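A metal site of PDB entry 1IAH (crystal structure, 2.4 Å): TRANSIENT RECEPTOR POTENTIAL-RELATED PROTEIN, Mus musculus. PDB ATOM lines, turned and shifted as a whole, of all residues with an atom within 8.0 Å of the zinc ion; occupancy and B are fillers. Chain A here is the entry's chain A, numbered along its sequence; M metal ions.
OE2 of Glu 187 lies within hydrogen-bond range of ND1 of His 260 (2.8 Å).
O of Pro 272 sits at hydrogen-bond distance from NE2 of His 203, 3.0 Å away.
The side-chain carboxylate (OE2) of Glu 207 sits at hydrogen-bond distance from a ring nitrogen (NE2) of His 203, 3.3 Å away.
The backbone NH (N) of Leu 271 lies within hydrogen-bond range of the backbone carbonyl oxygen (O) of Cys 266, at 3.0 Å.
The backbone NH (N) of Cys 266 lies within hydrogen-bond range of the side-chain amide oxygen (OD1) of Asn 263, 3.1 Å away.
Within 4 Å of the zinc ion: His 203, His 260, Cys 262 and Cys 266.
The nearest printed residue that does not touch the zinc ion is Leu 271 (4.6 Å).
The zinc ion is bound by a ring nitrogen (NE2) of His 260 (2.0 Å), a ring nitrogen (ND1) of His 203 (2.2 Å), the side-chain sulfur (SG) of Cys 266 (2.2 Å) and the side-chain sulfur (SG) of Cys 262 (2.4 Å).
The zinc ion has four donor atoms within binding distance.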
ATOM      1  N   GLU A 187      21.101  -5.302 -32.171  1.00  0.00           N
ATOM      2  CA  GLU A 187      19.872  -6.007 -32.428  1.00  0.00           C
ATOM      3  C   GLU A 187      18.713  -5.033 -32.406  1.00  0.00           C
ATOM      4  O   GLU A 187      18.786  -4.006 -31.728  1.00  0.00           O
ATOM      5  CB  GLU A 187      19.572  -7.036 -31.354  1.00  0.00           C
ATOM      6  CG  GLU A 187      20.699  -7.911 -30.947  1.00  0.00           C
ATOM      7  CD  GLU A 187      20.215  -8.947 -29.972  1.00  0.00           C
ATOM      8  OE1 GLU A 187      19.587  -8.558 -28.961  1.00  0.00           O
ATOM      9  OE2 GLU A 187      20.460 -10.141 -30.202  1.00  0.00           O
ATOM     10  N   GLU A 196      11.514 -11.957 -32.350  1.00  0.00           N
ATOM     11  CA  GLU A 196      12.086 -12.567 -31.160  1.00  0.00           C
ATOM     12  C   GLU A 196      12.758 -13.867 -31.590  1.00  0.00           C
ATOM     13  O   GLU A 196      13.939 -14.091 -31.288  1.00  0.00           O
ATOM     14  CB  GLU A 196      10.986 -12.901 -30.163  1.00  0.00           C
ATOM     15  CG  GLU A 196      10.592 -11.762 -29.250  1.00  0.00           C
ATOM     16  CD  GLU A 196       9.324 -12.071 -28.488  1.00  0.00           C
ATOM     17  OE1 GLU A 196       8.235 -11.979 -29.101  1.00  0.00           O
ATOM     18  OE2 GLU A 196       9.409 -12.426 -27.304  1.00  0.00           O
ATOM     19  N   LEU A 199      15.957 -13.275 -33.269  1.00  0.00           N
ATOM     20  CA  LEU A 199      17.002 -12.903 -32.335  1.00  0.00           C
ATOM     21  C   LEU A 199      17.467 -14.097 -31.537  1.00  0.00           C
ATOM     22  O   LEU A 199      18.659 -14.257 -31.280  1.00  0.00           O
ATOM     23  CB  LEU A 199      16.514 -11.788 -31.404  1.00  0.00           C
ATOM     24  CG  LEU A 199      16.189 -10.490 -32.159  1.00  0.00           C
ATOM     25  CD1 LEU A 199      15.736  -9.412 -31.169  1.00  0.00           C
ATOM     26  CD2 LEU A 199      17.419 -10.026 -32.952  1.00  0.00           C
ATOM     27  N   ALA A 200      16.532 -14.962 -31.160  1.00  0.00           N
ATOM     28  CA  ALA A 200      16.857 -16.149 -30.387  1.00  0.00           C
ATOM     29  C   ALA A 200      17.693 -17.105 -31.231  1.00  0.00           C
ATOM     30  O   ALA A 200      18.529 -17.840 -30.696  1.00  0.00           O
ATOM     31  CB  ALA A 200      15.582 -16.833 -29.922  1.00  0.00           C
ATOM     32  N   PHE A 201      17.474 -17.108 -32.533  1.00  0.00           N
ATOM     33  CA  PHE A 201      18.213 -18.006 -33.402  1.00  0.00           C
ATOM     34  C   PHE A 201      19.720 -17.823 -33.354  1.00  0.00           C
ATOM     35  O   PHE A 201      20.449 -18.797 -33.311  1.00  0.00           O
ATOM     36  CB  PHE A 201      17.763 -17.847 -34.853  1.00  0.00           C
ATOM     37  CG  PHE A 201      18.545 -18.696 -35.807  1.00  0.00           C
ATOM     38  CD1 PHE A 201      18.428 -20.088 -35.768  1.00  0.00           C
ATOM     39  CD2 PHE A 201      19.411 -18.115 -36.722  1.00  0.00           C
ATOM     40  CE1 PHE A 201      19.160 -20.896 -36.626  1.00  0.00           C
ATOM     41  CE2 PHE A 201      20.155 -18.919 -37.587  1.00  0.00           C
ATOM     42  CZ  PHE A 201      20.024 -20.305 -37.539  1.00  0.00           C
ATOM     43  N   SER A 202      20.175 -16.579 -33.399  1.00  0.00           N
ATOM     44  CA  SER A 202      21.609 -16.303 -33.371  1.00  0.00           C
ATOM     45  C   SER A 202      22.185 -16.793 -32.056  1.00  0.00           C
ATOM     46  O   SER A 202      23.317 -17.267 -31.996  1.00  0.00           O
ATOM     47  CB  SER A 202      21.865 -14.812 -33.537  1.00  0.00           C
ATOM     48  OG  SER A 202      21.544 -14.364 -34.847  1.00  0.00           O
ATOM     49  N   HIS A 203      21.403 -16.676 -30.998  1.00  0.00           N
ATOM     50  CA  HIS A 203      21.859 -17.116 -29.692  1.00  0.00           C
ATOM     51  C   HIS A 203      21.957 -18.632 -29.739  1.00  0.00           C
ATOM     52  O   HIS A 203      22.967 -19.216 -29.342  1.00  0.00           O
ATOM     53  CB  HIS A 203      20.855 -16.673 -28.622  1.00  0.00           C
ATOM     54  CG  HIS A 203      21.325 -16.953 -27.220  1.00  0.00           C
ATOM     55  ND1 HIS A 203      20.489 -16.791 -26.139  1.00  0.00           N
ATOM     56  CD2 HIS A 203      22.534 -17.386 -26.799  1.00  0.00           C
ATOM     57  CE1 HIS A 203      21.218 -17.137 -25.093  1.00  0.00           C
ATOM     58  NE2 HIS A 203      22.447 -17.502 -25.439  1.00  0.00           N
ATOM     59  N   TRP A 204      20.909 -19.253 -30.255  1.00  0.00           N
ATOM     60  CA  TRP A 204      20.856 -20.703 -30.366  1.00  0.00           C
ATOM     61  C   TRP A 204      22.027 -21.296 -31.159  1.00  0.00           C
ATOM     62  O   TRP A 204      22.582 -22.303 -30.747  1.00  0.00           O
ATOM     63  CB  TRP A 204      19.536 -21.121 -31.017  1.00  0.00           C
ATOM     64  CG  TRP A 204      19.388 -22.611 -31.230  1.00  0.00           C
ATOM     65  CD1 TRP A 204      18.822 -23.505 -30.360  1.00  0.00           C
ATOM     66  CD2 TRP A 204      19.784 -23.363 -32.378  1.00  0.00           C
ATOM     67  NE1 TRP A 204      18.842 -24.770 -30.914  1.00  0.00           N
ATOM     68  CE2 TRP A 204      19.437 -24.711 -32.141  1.00  0.00           C
ATOM     69  CE3 TRP A 204      20.405 -23.030 -33.593  1.00  0.00           C
ATOM     70  CZ2 TRP A 204      19.682 -25.729 -33.082  1.00  0.00           C
ATOM     71  CZ3 TRP A 204      20.656 -24.039 -34.520  1.00  0.00           C
ATOM     72  CH2 TRP A 204      20.290 -25.377 -34.252  1.00  0.00           C
ATOM     73  N   GLU A 207      25.120 -21.592 -28.824  1.00  0.00           N
ATOM     74  CA  GLU A 207      24.993 -22.658 -27.843  1.00  0.00           C
ATOM     75  C   GLU A 207      25.024 -24.021 -28.514  1.00  0.00           C
ATOM     76  O   GLU A 207      25.721 -24.934 -28.062  1.00  0.00           O
ATOM     77  CB  GLU A 207      23.694 -22.488 -27.057  1.00  0.00           C
ATOM     78  CG  GLU A 207      23.527 -21.136 -26.372  1.00  0.00           C
ATOM     79  CD  GLU A 207      24.553 -20.899 -25.267  1.00  0.00           C
ATOM     80  OE1 GLU A 207      25.129 -21.876 -24.738  1.00  0.00           O
ATOM     81  OE2 GLU A 207      24.772 -19.717 -24.920  1.00  0.00           O
ATOM     82  N   PHE A 256      28.673  -9.432 -29.151  1.00  0.00           N
ATOM     83  CA  PHE A 256      27.385 -10.081 -29.194  1.00  0.00           C
ATOM     84  C   PHE A 256      26.986 -10.601 -27.819  1.00  0.00           C
ATOM     85  O   PHE A 256      25.836 -10.482 -27.417  1.00  0.00           O
ATOM     86  CB  PHE A 256      27.354 -11.226 -30.199  1.00  0.00           C
ATOM     87  CG  PHE A 256      26.016 -11.863 -30.301  1.00  0.00           C
ATOM     88  CD1 PHE A 256      24.948 -11.152 -30.855  1.00  0.00           C
ATOM     89  CD2 PHE A 256      25.768 -13.124 -29.792  1.00  0.00           C
ATOM     90  CE1 PHE A 256      23.673 -11.684 -30.897  1.00  0.00           C
ATOM     91  CE2 PHE A 256      24.493 -13.679 -29.819  1.00  0.00           C
ATOM     92  CZ  PHE A 256      23.435 -12.955 -30.378  1.00  0.00           C
ATOM     93  N   HIS A 260      23.636  -8.778 -26.721  1.00  0.00           N
ATOM     94  CA  HIS A 260      22.431  -9.594 -26.875  1.00  0.00           C
ATOM     95  C   HIS A 260      21.505  -9.523 -25.656  1.00  0.00           C
ATOM     96  O   HIS A 260      21.961  -9.466 -24.517  1.00  0.00           O
ATOM     97  CB  HIS A 260      22.793 -11.056 -27.153  1.00  0.00           C
ATOM     98  CG  HIS A 260      21.610 -11.975 -27.152  1.00  0.00           C
ATOM     99  ND1 HIS A 260      20.586 -11.907 -28.073  1.00  0.00           N
ATOM    100  CD2 HIS A 260      21.279 -12.991 -26.311  1.00  0.00           C
ATOM    101  CE1 HIS A 260      19.677 -12.848 -27.752  1.00  0.00           C
ATOM    102  NE2 HIS A 260      20.073 -13.527 -26.698  1.00  0.00           N
ATOM    103  N   HIS A 261      20.206  -9.544 -25.907  1.00  0.00           N
ATOM    104  CA  HIS A 261      19.207  -9.493 -24.854  1.00  0.00           C
ATOM    105  C   HIS A 261      18.265 -10.677 -25.033  1.00  0.00           C
ATOM    106  O   HIS A 261      17.507 -10.733 -25.989  1.00  0.00           O
ATOM    107  CB  HIS A 261      18.428  -8.157 -24.930  1.00  0.00           C
ATOM    108  CG  HIS A 261      17.380  -8.003 -23.870  1.00  0.00           C
ATOM    109  ND1 HIS A 261      16.056  -8.321 -24.076  1.00  0.00           N
ATOM    110  CD2 HIS A 261      17.466  -7.597 -22.584  1.00  0.00           C
ATOM    111  CE1 HIS A 261      15.374  -8.122 -22.967  1.00  0.00           C
ATOM    112  NE2 HIS A 261      16.209  -7.679 -22.033  1.00  0.00           N
ATOM    113  N   CYS A 262      18.338 -11.654 -24.127  1.00  0.00           N
ATOM    114  CA  CYS A 262      17.481 -12.825 -24.234  1.00  0.00           C
ATOM    115  C   CYS A 262      16.016 -12.481 -24.065  1.00  0.00           C
ATOM    116  O   CYS A 262      15.660 -11.638 -23.243  1.00  0.00           O
ATOM    117  CB  CYS A 262      17.905 -13.889 -23.211  1.00  0.00           C
ATOM    118  SG  CYS A 262      19.535 -14.644 -23.539  1.00  0.00           S
ATOM    119  N   ASN A 263      15.159 -13.127 -24.856  1.00  0.00           N
ATOM    120  CA  ASN A 263      13.723 -12.893 -24.825  1.00  0.00           C
ATOM    121  C   ASN A 263      12.943 -14.157 -24.480  1.00  0.00           C
ATOM    122  O   ASN A 263      13.521 -15.183 -24.153  1.00  0.00           O
ATOM    123  CB  ASN A 263      13.246 -12.335 -26.168  1.00  0.00           C
ATOM    124  CG  ASN A 263      13.638 -13.219 -27.340  1.00  0.00           C
ATOM    125  OD1 ASN A 263      13.267 -14.395 -27.388  1.00  0.00           O
ATOM    126  ND2 ASN A 263      14.378 -12.658 -28.284  1.00  0.00           N
ATOM    127  N   SER A 264      11.617 -14.065 -24.559  1.00  0.00           N
ATOM    128  CA  SER A 264      10.773 -15.209 -24.248  1.00  0.00           C
ATOM    129  C   SER A 264      11.093 -16.417 -25.108  1.00  0.00           C
ATOM    130  O   SER A 264      10.803 -17.556 -24.722  1.00  0.00           O
ATOM    131  CB  SER A 264       9.297 -14.838 -24.410  1.00  0.00           C
ATOM    132  OG  SER A 264       8.998 -14.532 -25.762  1.00  0.00           O
ATOM    133  N   CYS A 265      11.669 -16.185 -26.283  1.00  0.00           N
ATOM    134  CA  CYS A 265      12.007 -17.293 -27.156  1.00  0.00           C
ATOM    135  C   CYS A 265      13.275 -17.962 -26.649  1.00  0.00           C
ATOM    136  O   CYS A 265      13.354 -19.192 -26.584  1.00  0.00           O
ATOM    137  CB  CYS A 265      12.210 -16.821 -28.592  1.00  0.00           C
ATOM    138  SG  CYS A 265      12.274 -18.181 -29.771  1.00  0.00           S
ATOM    139  N   CYS A 266      14.256 -17.154 -26.286  1.00  0.00           N
ATOM    140  CA  CYS A 266      15.511 -17.667 -25.741  1.00  0.00           C
ATOM    141  C   CYS A 266      15.195 -18.556 -24.560  1.00  0.00           C
ATOM    142  O   CYS A 266      15.774 -19.620 -24.390  1.00  0.00           O
ATOM    143  CB  CYS A 266      16.403 -16.526 -25.268  1.00  0.00           C
ATOM    144  SG  CYS A 266      17.066 -15.510 -26.602  1.00  0.00           S
ATOM    145  N   ARG A 267      14.274 -18.085 -23.730  1.00  0.00           N
ATOM    146  CA  ARG A 267      13.868 -18.806 -22.544  1.00  0.00           C
ATOM    147  C   ARG A 267      13.101 -20.062 -22.940  1.00  0.00           C
ATOM    148  O   ARG A 267      13.305 -21.128 -22.358  1.00  0.00           O
ATOM    149  CB  ARG A 267      13.017 -17.907 -21.644  1.00  0.00           C
ATOM    150  CG  ARG A 267      13.820 -17.196 -20.532  1.00  0.00           C
ATOM    151  CD  ARG A 267      13.602 -15.680 -20.507  1.00  0.00           C
ATOM    152  NE  ARG A 267      12.190 -15.336 -20.433  1.00  0.00           N
ATOM    153  CZ  ARG A 267      11.677 -14.179 -20.819  1.00  0.00           C
ATOM    154  NH1 ARG A 267      12.469 -13.236 -21.308  1.00  0.00           N
ATOM    155  NH2 ARG A 267      10.372 -13.952 -20.723  1.00  0.00           N
ATOM    156  N   LEU A 269      13.573 -21.711 -25.460  1.00  0.00           N
ATOM    157  CA  LEU A 269      14.620 -22.593 -25.963  1.00  0.00           C
ATOM    158  C   LEU A 269      15.572 -23.050 -24.862  1.00  0.00           C
ATOM    159  O   LEU A 269      16.508 -23.802 -25.110  1.00  0.00           O
ATOM    160  CB  LEU A 269      15.420 -21.885 -27.046  1.00  0.00           C
ATOM    161  CG  LEU A 269      14.651 -21.638 -28.346  1.00  0.00           C
ATOM    162  CD1 LEU A 269      15.402 -20.610 -29.167  1.00  0.00           C
ATOM    163  CD2 LEU A 269      14.479 -22.960 -29.108  1.00  0.00           C
ATOM    164  N   LEU A 271      17.883 -21.479 -23.411  1.00  0.00           N
ATOM    165  CA  LEU A 271      19.257 -21.047 -23.680  1.00  0.00           C
ATOM    166  C   LEU A 271      19.896 -20.349 -22.477  1.00  0.00           C
ATOM    167  O   LEU A 271      19.278 -19.502 -21.829  1.00  0.00           O
ATOM    168  CB  LEU A 271      19.299 -20.107 -24.879  1.00  0.00           C
ATOM    169  CG  LEU A 271      18.643 -20.558 -26.179  1.00  0.00           C
ATOM    170  CD1 LEU A 271      18.809 -19.460 -27.219  1.00  0.00           C
ATOM    171  CD2 LEU A 271      19.264 -21.858 -26.660  1.00  0.00           C
ATOM    172  N   PRO A 272      21.156 -20.683 -22.168  1.00  0.00           N
ATOM    173  CA  PRO A 272      21.882 -20.085 -21.047  1.00  0.00           C
ATOM    174  C   PRO A 272      22.295 -18.656 -21.356  1.00  0.00           C
ATOM    175  O   PRO A 272      22.377 -18.281 -22.514  1.00  0.00           O
ATOM    176  CB  PRO A 272      23.103 -20.990 -20.892  1.00  0.00           C
ATOM    177  CG  PRO A 272      22.719 -22.269 -21.578  1.00  0.00           C
ATOM    178  CD  PRO A 272      21.907 -21.809 -22.747  1.00  0.00           C
ATOM    179  N   ASP A 273      22.586 -17.879 -20.323  1.00  0.00           N
ATOM    180  CA  ASP A 273      23.012 -16.503 -20.517  1.00  0.00           C
ATOM    181  C   ASP A 273      24.371 -16.461 -21.216  1.00  0.00           C
ATOM    182  O   ASP A 273      25.300 -17.150 -20.798  1.00  0.00           O
ATOM    183  CB  ASP A 273      23.107 -15.770 -19.187  1.00  0.00           C
ATOM    184  CG  ASP A 273      23.038 -14.266 -19.347  1.00  0.00           C
ATOM    185  OD1 ASP A 273      21.917 -13.724 -19.324  1.00  0.00           O
ATOM    186  OD2 ASP A 273      24.106 -13.639 -19.509  1.00  0.00           O
ATOM    187  N   LEU A 274      24.482 -15.656 -22.258  1.00  0.00           N
ATOM    188  CA  LEU A 274      25.736 -15.543 -23.000  1.00  0.00           C
ATOM    189  C   LEU A 274      26.846 -14.878 -22.198  1.00  0.00           C
ATOM    190  O   LEU A 274      28.014 -14.959 -22.566  1.00  0.00           O
ATOM    191  CB  LEU A 274      25.532 -14.725 -24.265  1.00  0.00           C
ATOM    192  CG  LEU A 274      24.754 -15.460 -25.337  1.00  0.00           C
ATOM    193  CD1 LEU A 274      24.550 -14.516 -26.507  1.00  0.00           C
ATOM    194  CD2 LEU A 274      25.508 -16.715 -25.749  1.00  0.00           C
HETATM  195 ZN    ZN M   1      19.138 -15.120 -25.858  1.00  0.00          ZN
